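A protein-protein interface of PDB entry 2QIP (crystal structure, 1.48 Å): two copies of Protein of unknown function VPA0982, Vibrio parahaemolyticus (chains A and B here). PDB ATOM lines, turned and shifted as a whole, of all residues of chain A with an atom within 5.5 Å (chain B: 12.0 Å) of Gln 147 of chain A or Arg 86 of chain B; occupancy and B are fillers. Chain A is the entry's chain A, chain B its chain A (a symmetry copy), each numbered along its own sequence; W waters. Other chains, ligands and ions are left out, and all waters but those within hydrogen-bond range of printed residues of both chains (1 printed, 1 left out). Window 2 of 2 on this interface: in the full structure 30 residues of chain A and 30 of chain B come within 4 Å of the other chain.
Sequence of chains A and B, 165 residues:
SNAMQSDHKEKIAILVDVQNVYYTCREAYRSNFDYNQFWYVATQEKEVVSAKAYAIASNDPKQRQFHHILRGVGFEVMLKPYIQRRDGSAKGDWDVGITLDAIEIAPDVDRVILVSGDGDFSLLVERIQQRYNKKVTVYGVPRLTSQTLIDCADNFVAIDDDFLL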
ATOM      1  N   PRO A 142     -22.969  -9.615  26.843  1.00  0.00           N
ATOM      2  CA  PRO A 142     -22.352 -10.910  26.478  1.00  0.00           C
ATOM      3  C   PRO A 142     -23.234 -11.850  25.662  1.00  0.00           C
ATOM      4  O   PRO A 142     -22.754 -12.416  24.671  1.00  0.00           O
ATOM      5  CB  PRO A 142     -21.977 -11.521  27.825  1.00  0.00           C
ATOM      6  CG  PRO A 142     -21.763 -10.348  28.700  1.00  0.00           C
ATOM      7  CD  PRO A 142     -22.834  -9.344  28.287  1.00  0.00           C
ATOM      8  N   ARG A 143     -24.507 -11.981  26.032  1.00  0.00           N
ATOM      9  CA  ARG A 143     -25.365 -12.964  25.360  1.00  0.00           C
ATOM     10  C   ARG A 143     -25.733 -12.543  23.921  1.00  0.00           C
ATOM     11  O   ARG A 143     -26.312 -13.316  23.161  1.00  0.00           O
ATOM     12  CB  ARG A 143     -26.590 -13.326  26.233  1.00  0.00           C
ATOM     13  CG  ARG A 143     -27.640 -12.237  26.354  1.00  0.00           C
ATOM     14  CD  ARG A 143     -28.764 -12.582  27.365  1.00  0.00           C
ATOM     15  NE  ARG A 143     -28.466 -12.160  28.741  1.00  0.00           N
ATOM     16  CZ  ARG A 143     -28.067 -12.976  29.718  1.00  0.00           C
ATOM     17  NH1 ARG A 143     -27.834 -12.500  30.940  1.00  0.00           N
ATOM     18  NH2 ARG A 143     -27.903 -14.276  29.485  1.00  0.00           N
ATOM     19  N   LEU A 144     -25.342 -11.330  23.529  1.00  0.00           N
ATOM     20  CA  LEU A 144     -25.661 -10.805  22.200  1.00  0.00           C
ATOM     21  C   LEU A 144     -24.436 -10.281  21.465  1.00  0.00           C
ATOM     22  O   LEU A 144     -24.571  -9.688  20.395  1.00  0.00           O
ATOM     23  CB  LEU A 144     -26.748  -9.723  22.295  1.00  0.00           C
ATOM     24  CG  LEU A 144     -28.113 -10.256  22.785  1.00  0.00           C
ATOM     25  CD1 LEU A 144     -29.071  -9.117  23.113  1.00  0.00           C
ATOM     26  CD2 LEU A 144     -28.735 -11.214  21.763  1.00  0.00           C
ATOM     27  N   THR A 145     -23.262 -10.528  22.038  1.00  0.00           N
ATOM     28  CA  THR A 145     -21.990 -10.102  21.444  1.00  0.00           C
ATOM     29  C   THR A 145     -21.309 -11.259  20.738  1.00  0.00           C
ATOM     30  O   THR A 145     -21.225 -12.377  21.267  1.00  0.00           O
ATOM     31  CB  THR A 145     -21.042  -9.535  22.512  1.00  0.00           C
ATOM     32  OG1 THR A 145     -21.626  -8.347  23.054  1.00  0.00           O
ATOM     33  CG2 THR A 145     -19.676  -9.163  21.936  1.00  0.00           C
ATOM     34  N   SER A 146     -20.817 -10.987  19.535  1.00  0.00           N
ATOM     35  CA  SER A 146     -20.106 -11.998  18.769  1.00  0.00           C
ATOM     36  C   SER A 146     -18.899 -12.531  19.503  1.00  0.00           C
ATOM     37  O   SER A 146     -18.068 -11.733  19.944  1.00  0.00           O
ATOM     38  CB  SER A 146     -19.621 -11.349  17.489  1.00  0.00           C
ATOM     39  OG  SER A 146     -18.763 -12.210  16.781  1.00  0.00           O
ATOM     40  N   GLN A 147     -18.739 -13.856  19.567  1.00  0.00           N
ATOM     41  CA  GLN A 147     -17.558 -14.438  20.211  1.00  0.00           C
ATOM     42  C   GLN A 147     -16.272 -14.064  19.461  1.00  0.00           C
ATOM     43  O   GLN A 147     -15.194 -13.933  20.065  1.00  0.00           O
ATOM     44  CB  GLN A 147     -17.663 -15.976  20.369  1.00  0.00           C
ATOM     45  CG  GLN A 147     -16.587 -16.548  21.272  1.00  0.00           C
ATOM     46  CD  GLN A 147     -16.675 -16.020  22.703  1.00  0.00           C
ATOM     47  OE1 GLN A 147     -17.766 -15.925  23.275  1.00  0.00           O
ATOM     48  NE2 GLN A 147     -15.531 -15.671  23.281  1.00  0.00           N
ATOM     49  N   THR A 148     -16.390 -13.878  18.145  1.00  0.00           N
ATOM     50  CA  THR A 148     -15.224 -13.516  17.339  1.00  0.00           C
ATOM     51  C   THR A 148     -14.724 -12.138  17.749  1.00  0.00           C
ATOM     52  O   THR A 148     -13.522 -11.927  17.859  1.00  0.00           O
ATOM     53  CB  THR A 148     -15.605 -13.536  15.851  1.00  0.00           C
ATOM     54  OG1 THR A 148     -16.148 -14.835  15.530  1.00  0.00           O
ATOM     55  CG2 THR A 148     -14.429 -13.227  14.955  1.00  0.00           C
ATOM     56  N   LEU A 149     -15.655 -11.214  17.987  1.00  0.00           N
ATOM     57  CA  LEU A 149     -15.288  -9.877  18.447  1.00  0.00           C
ATOM     58  C   LEU A 149     -14.650  -9.915  19.836  1.00  0.00           C
ATOM     59  O   LEU A 149     -13.622  -9.263  20.067  1.00  0.00           O
ATOM     60  CB  LEU A 149     -16.531  -8.974  18.457  1.00  0.00           C
ATOM     61  CG  LEU A 149     -16.336  -7.516  18.906  1.00  0.00           C
ATOM     62  CD1 LEU A 149     -15.386  -6.810  17.979  1.00  0.00           C
ATOM     63  CD2 LEU A 149     -17.660  -6.772  18.933  1.00  0.00           C
ATOM     64  N   ILE A 150     -15.230 -10.703  20.745  1.00  0.00           N
ATOM     65  CA  ILE A 150     -14.674 -10.855  22.099  1.00  0.00           C
ATOM     66  C   ILE A 150     -13.244 -11.386  22.025  1.00  0.00           C
ATOM     67  O   ILE A 150     -12.346 -10.863  22.686  1.00  0.00           O
ATOM     68  CB  ILE A 150     -15.566 -11.802  22.957  1.00  0.00           C
ATOM     69  CG1 ILE A 150     -16.913 -11.126  23.248  1.00  0.00           C
ATOM     70  CG2 ILE A 150     -14.871 -12.171  24.276  1.00  0.00           C
ATOM     71  CD1 ILE A 150     -17.939 -12.047  23.888  1.00  0.00           C
ATOM     72  N   ASP A 151     -13.020 -12.382  21.170  1.00  0.00           N
ATOM     73  CA  ASP A 151     -11.702 -13.020  21.081  1.00  0.00           C
ATOM     74  C   ASP A 151     -10.673 -12.121  20.393  1.00  0.00           C
ATOM     75  O   ASP A 151      -9.485 -12.202  20.693  1.00  0.00           O
ATOM     76  CB  ASP A 151     -11.830 -14.342  20.326  1.00  0.00           C
ATOM     77  CG  ASP A 151     -12.569 -15.414  21.144  1.00  0.00           C
ATOM     78  OD1 ASP A 151     -12.780 -15.218  22.362  1.00  0.00           O
ATOM     79  OD2 ASP A 151     -12.942 -16.445  20.562  1.00  0.00           O
ATOM     80  N   CYS A 152     -11.127 -11.275  19.457  1.00  0.00           N
ATOM     81  CA  CYS A 152     -10.222 -10.350  18.755  1.00  0.00           C
ATOM     82  C   CYS A 152      -9.739  -9.241  19.703  1.00  0.00           C
ATOM     83  O   CYS A 152      -8.593  -8.807  19.609  1.00  0.00           O
ATOM     84  CB  CYS A 152     -10.927  -9.699  17.545  1.00  0.00           C
ATOM     85  SG  CYS A 152     -11.095 -10.775  16.137  1.00  0.00           S
ATOM     86  N   LYS B  80     -15.201 -13.492   3.149  1.00  0.00           N
ATOM     87  CA  LYS B  80     -15.439 -12.961   4.477  1.00  0.00           C
ATOM     88  C   LYS B  80     -14.979 -13.944   5.559  1.00  0.00           C
ATOM     89  O   LYS B  80     -15.325 -15.131   5.503  1.00  0.00           O
ATOM     90  CB  LYS B  80     -16.907 -12.588   4.667  1.00  0.00           C
ATOM     91  CG  LYS B  80     -17.091 -11.766   5.920  1.00  0.00           C
ATOM     92  CD  LYS B  80     -18.474 -11.220   6.063  1.00  0.00           C
ATOM     93  CE  LYS B  80     -18.527 -10.295   7.277  1.00  0.00           C
ATOM     94  NZ  LYS B  80     -19.919  -9.924   7.579  1.00  0.00           N
ATOM     95  N   PRO B  81     -14.179 -13.464   6.530  1.00  0.00           N
ATOM     96  CA  PRO B  81     -13.840 -14.354   7.641  1.00  0.00           C
ATOM     97  C   PRO B  81     -15.083 -14.772   8.409  1.00  0.00           C
ATOM     98  O   PRO B  81     -16.028 -14.001   8.536  1.00  0.00           O
ATOM     99  CB  PRO B  81     -12.968 -13.476   8.549  1.00  0.00           C
ATOM    100  CG  PRO B  81     -12.514 -12.320   7.679  1.00  0.00           C
ATOM    101  CD  PRO B  81     -13.554 -12.129   6.654  1.00  0.00           C
ATOM    102  N   TYR B  82     -15.046 -15.991   8.937  1.00  0.00           N
ATOM    103  CA  TYR B  82     -16.046 -16.445   9.895  1.00  0.00           C
ATOM    104  C   TYR B  82     -16.251 -15.426  11.025  1.00  0.00           C
ATOM    105  O   TYR B  82     -15.293 -14.946  11.645  1.00  0.00           O
ATOM    106  CB  TYR B  82     -15.594 -17.773  10.506  1.00  0.00           C
ATOM    107  CG  TYR B  82     -16.433 -18.182  11.697  1.00  0.00           C
ATOM    108  CD1 TYR B  82     -17.753 -18.593  11.527  1.00  0.00           C
ATOM    109  CD2 TYR B  82     -15.902 -18.149  12.997  1.00  0.00           C
ATOM    110  CE1 TYR B  82     -18.545 -18.958  12.625  1.00  0.00           C
ATOM    111  CE2 TYR B  82     -16.682 -18.521  14.102  1.00  0.00           C
ATOM    112  CZ  TYR B  82     -18.004 -18.917  13.896  1.00  0.00           C
ATOM    113  OH  TYR B  82     -18.788 -19.305  14.969  1.00  0.00           O
ATOM    114  N   ILE B  83     -17.510 -15.142  11.321  1.00  0.00           N
ATOM    115  CA  ILE B  83     -17.830 -14.262  12.444  1.00  0.00           C
ATOM    116  C   ILE B  83     -18.991 -14.887  13.190  1.00  0.00           C
ATOM    117  O   ILE B  83     -20.078 -15.021  12.641  1.00  0.00           O
ATOM    118  CB  ILE B  83     -18.182 -12.812  11.984  1.00  0.00           C
ATOM    119  CG1 ILE B  83     -16.947 -12.127  11.358  1.00  0.00           C
ATOM    120  CG2 ILE B  83     -18.700 -11.994  13.180  1.00  0.00           C
ATOM    121  CD1 ILE B  83     -17.188 -10.775  10.737  1.00  0.00           C
ATOM    122  N   GLN B  84     -18.734 -15.274  14.438  1.00  0.00           N
ATOM    123  CA  GLN B  84     -19.759 -15.874  15.290  1.00  0.00           C
ATOM    124  C   GLN B  84     -20.881 -14.864  15.552  1.00  0.00           C
ATOM    125  O   GLN B  84     -20.632 -13.677  15.723  1.00  0.00           O
ATOM    126  CB  GLN B  84     -19.111 -16.329  16.598  1.00  0.00           C
ATOM    127  CG  GLN B  84     -19.924 -17.340  17.393  1.00  0.00           C
ATOM    128  CD  GLN B  84     -20.990 -16.699  18.275  1.00  0.00           C
ATOM    129  OE1 GLN B  84     -20.864 -15.552  18.728  1.00  0.00           O
ATOM    130  NE2 GLN B  84     -22.061 -17.444  18.524  1.00  0.00           N
ATOM    131  N   ARG B  85     -22.121 -15.336  15.587  1.00  0.00           N
ATOM    132  CA  ARG B  85     -23.258 -14.430  15.734  1.00  0.00           C
ATOM    133  C   ARG B  85     -24.166 -14.892  16.871  1.00  0.00           C
ATOM    134  O   ARG B  85     -24.569 -16.057  16.903  1.00  0.00           O
ATOM    135  CB  ARG B  85     -24.032 -14.367  14.410  1.00  0.00           C
ATOM    136  CG  ARG B  85     -25.092 -13.292  14.327  1.00  0.00           C
ATOM    137  CD  ARG B  85     -26.463 -13.905  14.089  1.00  0.00           C
ATOM    138  NE  ARG B  85     -26.752 -14.238  12.693  1.00  0.00           N
ATOM    139  CZ  ARG B  85     -27.817 -14.930  12.284  1.00  0.00           C
ATOM    140  NH1 ARG B  85     -28.707 -15.392  13.160  1.00  0.00           N
ATOM    141  NH2 ARG B  85     -27.993 -15.170  10.991  1.00  0.00           N
ATOM    142  N   ARG B  86     -24.473 -13.975  17.792  1.00  0.00           N
ATOM    143  CA  ARG B  86     -25.376 -14.254  18.921  1.00  0.00           C
ATOM    144  C   ARG B  86     -26.665 -13.429  18.853  1.00  0.00           C
ATOM    145  O   ARG B  86     -27.645 -13.761  19.524  1.00  0.00           O
ATOM    146  CB  ARG B  86     -24.676 -13.990  20.268  1.00  0.00           C
ATOM    147  CG  ARG B  86     -23.720 -15.084  20.707  1.00  0.00           C
ATOM    148  CD  ARG B  86     -23.270 -14.918  22.152  1.00  0.00           C
ATOM    149  NE  ARG B  86     -22.393 -16.024  22.556  1.00  0.00           N
ATOM    150  CZ  ARG B  86     -21.077 -15.934  22.735  1.00  0.00           C
ATOM    151  NH1 ARG B  86     -20.442 -14.772  22.590  1.00  0.00           N
ATOM    152  NH2 ARG B  86     -20.387 -17.014  23.093  1.00  0.00           N
ATOM    153  N   ASP B  87     -26.667 -12.370  18.042  1.00  0.00           N
ATOM    154  CA  ASP B  87     -27.752 -11.373  18.055  1.00  0.00           C
ATOM    155  C   ASP B  87     -28.841 -11.551  16.984  1.00  0.00           C
ATOM    156  O   ASP B  87     -29.806 -10.772  16.936  1.00  0.00           O
ATOM    157  CB  ASP B  87     -27.167  -9.952  17.974  1.00  0.00           C
ATOM    158  CG  ASP B  87     -26.309  -9.730  16.726  1.00  0.00           C
ATOM    159  OD1 ASP B  87     -26.306 -10.593  15.823  1.00  0.00           O
ATOM    160  OD2 ASP B  87     -25.627  -8.682  16.647  1.00  0.00           O
ATOM    161  N   GLY B  88     -28.682 -12.558  16.127  1.00  0.00           N
ATOM    162  CA  GLY B  88     -29.641 -12.814  15.046  1.00  0.00           C
ATOM    163  C   GLY B  88     -29.520 -11.893  13.838  1.00  0.00           C
ATOM    164  O   GLY B  88     -30.399 -11.883  12.970  1.00  0.00           O
ATOM    165  N   SER B  89     -28.434 -11.127  13.769  1.00  0.00           N
ATOM    166  CA  SER B  89     -28.216 -10.157  12.685  1.00  0.00           C
ATOM    167  C   SER B  89     -27.695 -10.807  11.394  1.00  0.00           C
ATOM    168  O   SER B  89     -27.238 -11.948  11.404  1.00  0.00           O
ATOM    169  CB  SER B  89     -27.245  -9.067  13.148  1.00  0.00           C
ATOM    170  OG  SER B  89     -25.967  -9.620  13.434  1.00  0.00           O
ATOM    171  N   ALA B  90     -27.756 -10.059  10.290  1.00  0.00           N
ATOM    172  CA  ALA B  90     -27.315 -10.538   8.975  1.00  0.00           C
ATOM    173  C   ALA B  90     -25.819 -10.868   8.940  1.00  0.00           C
ATOM    174  O   ALA B  90     -24.987 -10.035   9.308  1.00  0.00           O
ATOM    175  CB  ALA B  90     -27.657  -9.506   7.907  1.00  0.00           C
ATOM    176  N   LYS B  91     -25.491 -12.080   8.485  1.00  0.00           N
ATOM    177  CA  LYS B  91     -24.098 -12.564   8.446  1.00  0.00           C
ATOM    178  C   LYS B  91     -23.286 -12.066   7.238  1.00  0.00           C
ATOM    179  O   LYS B  91     -22.054 -12.135   7.236  1.00  0.00           O
ATOM    180  CB  LYS B  91     -24.057 -14.096   8.446  1.00  0.00           C
ATOM    181  CG  LYS B  91     -24.726 -14.779   9.632  1.00  0.00           C
ATOM    182  CD  LYS B  91     -24.498 -16.289   9.551  1.00  0.00           C
ATOM    183  CE  LYS B  91     -25.444 -17.075  10.457  1.00  0.00           C
ATOM    184  NZ  LYS B  91     -25.134 -16.908  11.906  1.00  0.00           N
ATOM    185  N   GLY B  92     -23.969 -11.570   6.211  1.00  0.00           N
ATOM    186  CA  GLY B  92     -23.321 -11.345   4.928  1.00  0.00           C
ATOM    187  C   GLY B  92     -22.652 -10.006   4.670  1.00  0.00           C
ATOM    188  O   GLY B  92     -22.127  -9.798   3.561  1.00  0.00           O
HETATM  189  O   HOH W   1     -24.968  -7.354  18.851  1.00  0.00           O
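Hydrophobic or aromatic side chains of chain B within 4 Å of the printed part of chain A: Tyr 82 and Ile 83.
Of the 11 printed residues of chain A, 8 touch a printed residue of chain B.
Printed residues of chain A that touch a printed residue of chain B: Pro 142, Arg 143, Leu 144, Thr 145, Ser 146, Gln 147, Thr 148 and Ile 150.
Along chain A the printed residues that touch a printed residue of chain B span positions 142 to 150.
Among the printed residues, 13 pairs touch across the chains.
Among the printed residues, no Asp or Glu carboxylate lies within 4 Å of a Lys or Arg side-chain nitrogen of the other chain.
No position is printed for both chains.
Of the 13 pairs that touch across the chains among the printed residues, none has its exchanged pair printed and touching as well.
Water W1 bridges OD2 of Asp 87 of chain B (2.7 Å) and O of Leu 144 of chain A (2.8 Å).
Pro 142 of chain A touches Arg 86 of chain B (O to CD, 3.6 Å).
O of Arg 143 of chain A touches CB of Arg 86 of chain B, at 3.4 Å.
Leu 144 of chain A touches Arg 86 of chain B (CD2 to O, 3.6 Å).
Leu 144 of chain A touches Asp 87 of chain B.
Ser 146 of chain A touches Ile 83 of chain B (OG to CG2, 3.6 Å).
Thr 148 of chain A touches Tyr 82 of chain B.
CA of Ile 83 of chain B touches OG1 of Thr 148 of chain A (3.6 Å).
Ile 150 of chain A touches Arg 86 of chain B.
Printed residues of chain B within 4 Å of Pro 142 of chain A: Arg 86 (3.6 Å).
Printed residues of chain B within 4 Å of Arg 143 of chain A: Arg 86 (3.4 Å).
Leu 144 of chain A touches just these residues of chain B: Arg 86 (3.6 Å) and Asp 87 (3.6 Å).
Thr 145 of chain A touches one residue of chain B.
Of chain B, only Ile 83 and Gln 84 come within 4 Å of Ser 146 of chain A.
Gln 147 of chain A touches just these residues of chain B: Gln 84 and Arg 86.
Of chain B, only Tyr 82 (3.8 Å), Ile 83 (3.6 Å) and Gln 84 (2.8 Å) come within 4 Å of Thr 148 of chain A.
No residue of chain B comes within 4 Å of Leu 149 of chain A.
No residue of chain B comes within 4 Å of Asp 151 of chain A.
Cys 152 of chain A touches none of the printed residues of chain B.
Of the printed residues of chain A, Tyr 82 of chain B touches Thr 148 (3.8 Å).
Of the printed residues of chain A, Gln 84 of chain B touches Ser 146 (2.6 Å), Gln 147 (2.8 Å) and Thr 148 (2.8 Å).
Arg 86 of chain B touches six residues of chain A.
The nearest residue of chain B that does not touch Gln 147 of chain A is Arg 85 of chain B (5.4 Å).
The backbone carbonyl oxygen of Thr 148 of chain A sits at hydrogen-bond distance from the side-chain sulfur of Cys 152 of chain A, at 3.2 Å.
The side-chain hydroxyl (OG) of Ser 146 of chain A is in hydrogen-bond range of the backbone NH (N) of Leu 149 of chain A, at 3.5 Å.
OD1 of Asp 151 of chain A sits at hydrogen-bond distance from NE2 of Gln 147 of chain A (2.9 Å).
The side-chain hydroxyl (OG) of Ser 146 of chain A sits close to the backbone NH (N) of Thr 148 of chain A (3.2 Å).
The side-chain hydroxyl (OG) of Ser 89 of chain B is in hydrogen-bond range of the side-chain carboxylate (OD1) of Asp 87 of chain B (2.6 Å).
The side-chain amide oxygen (OE1) of Gln 84 of chain B lies within hydrogen-bond range of the backbone NH (N) of Gln 147 of chain A, 2.8 Å away.
The side-chain hydroxyl (OG) of Ser 146 of chain A sits at hydrogen-bond distance from the backbone carbonyl oxygen (O) of Gln 84 of chain B.
NH2 of Arg 86 of chain B is in hydrogen-bond range of OE1 of Gln 147 of chain A (2.8 Å).
NH1 of Arg 86 of chain B sits at hydrogen-bond distance from O of Thr 145 of chain A, at 2.8 Å.
The side-chain hydroxyl of Thr 148 of chain A lies within hydrogen-bond range of the backbone NH of Gln 84 of chain B, at 2.8 Å.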
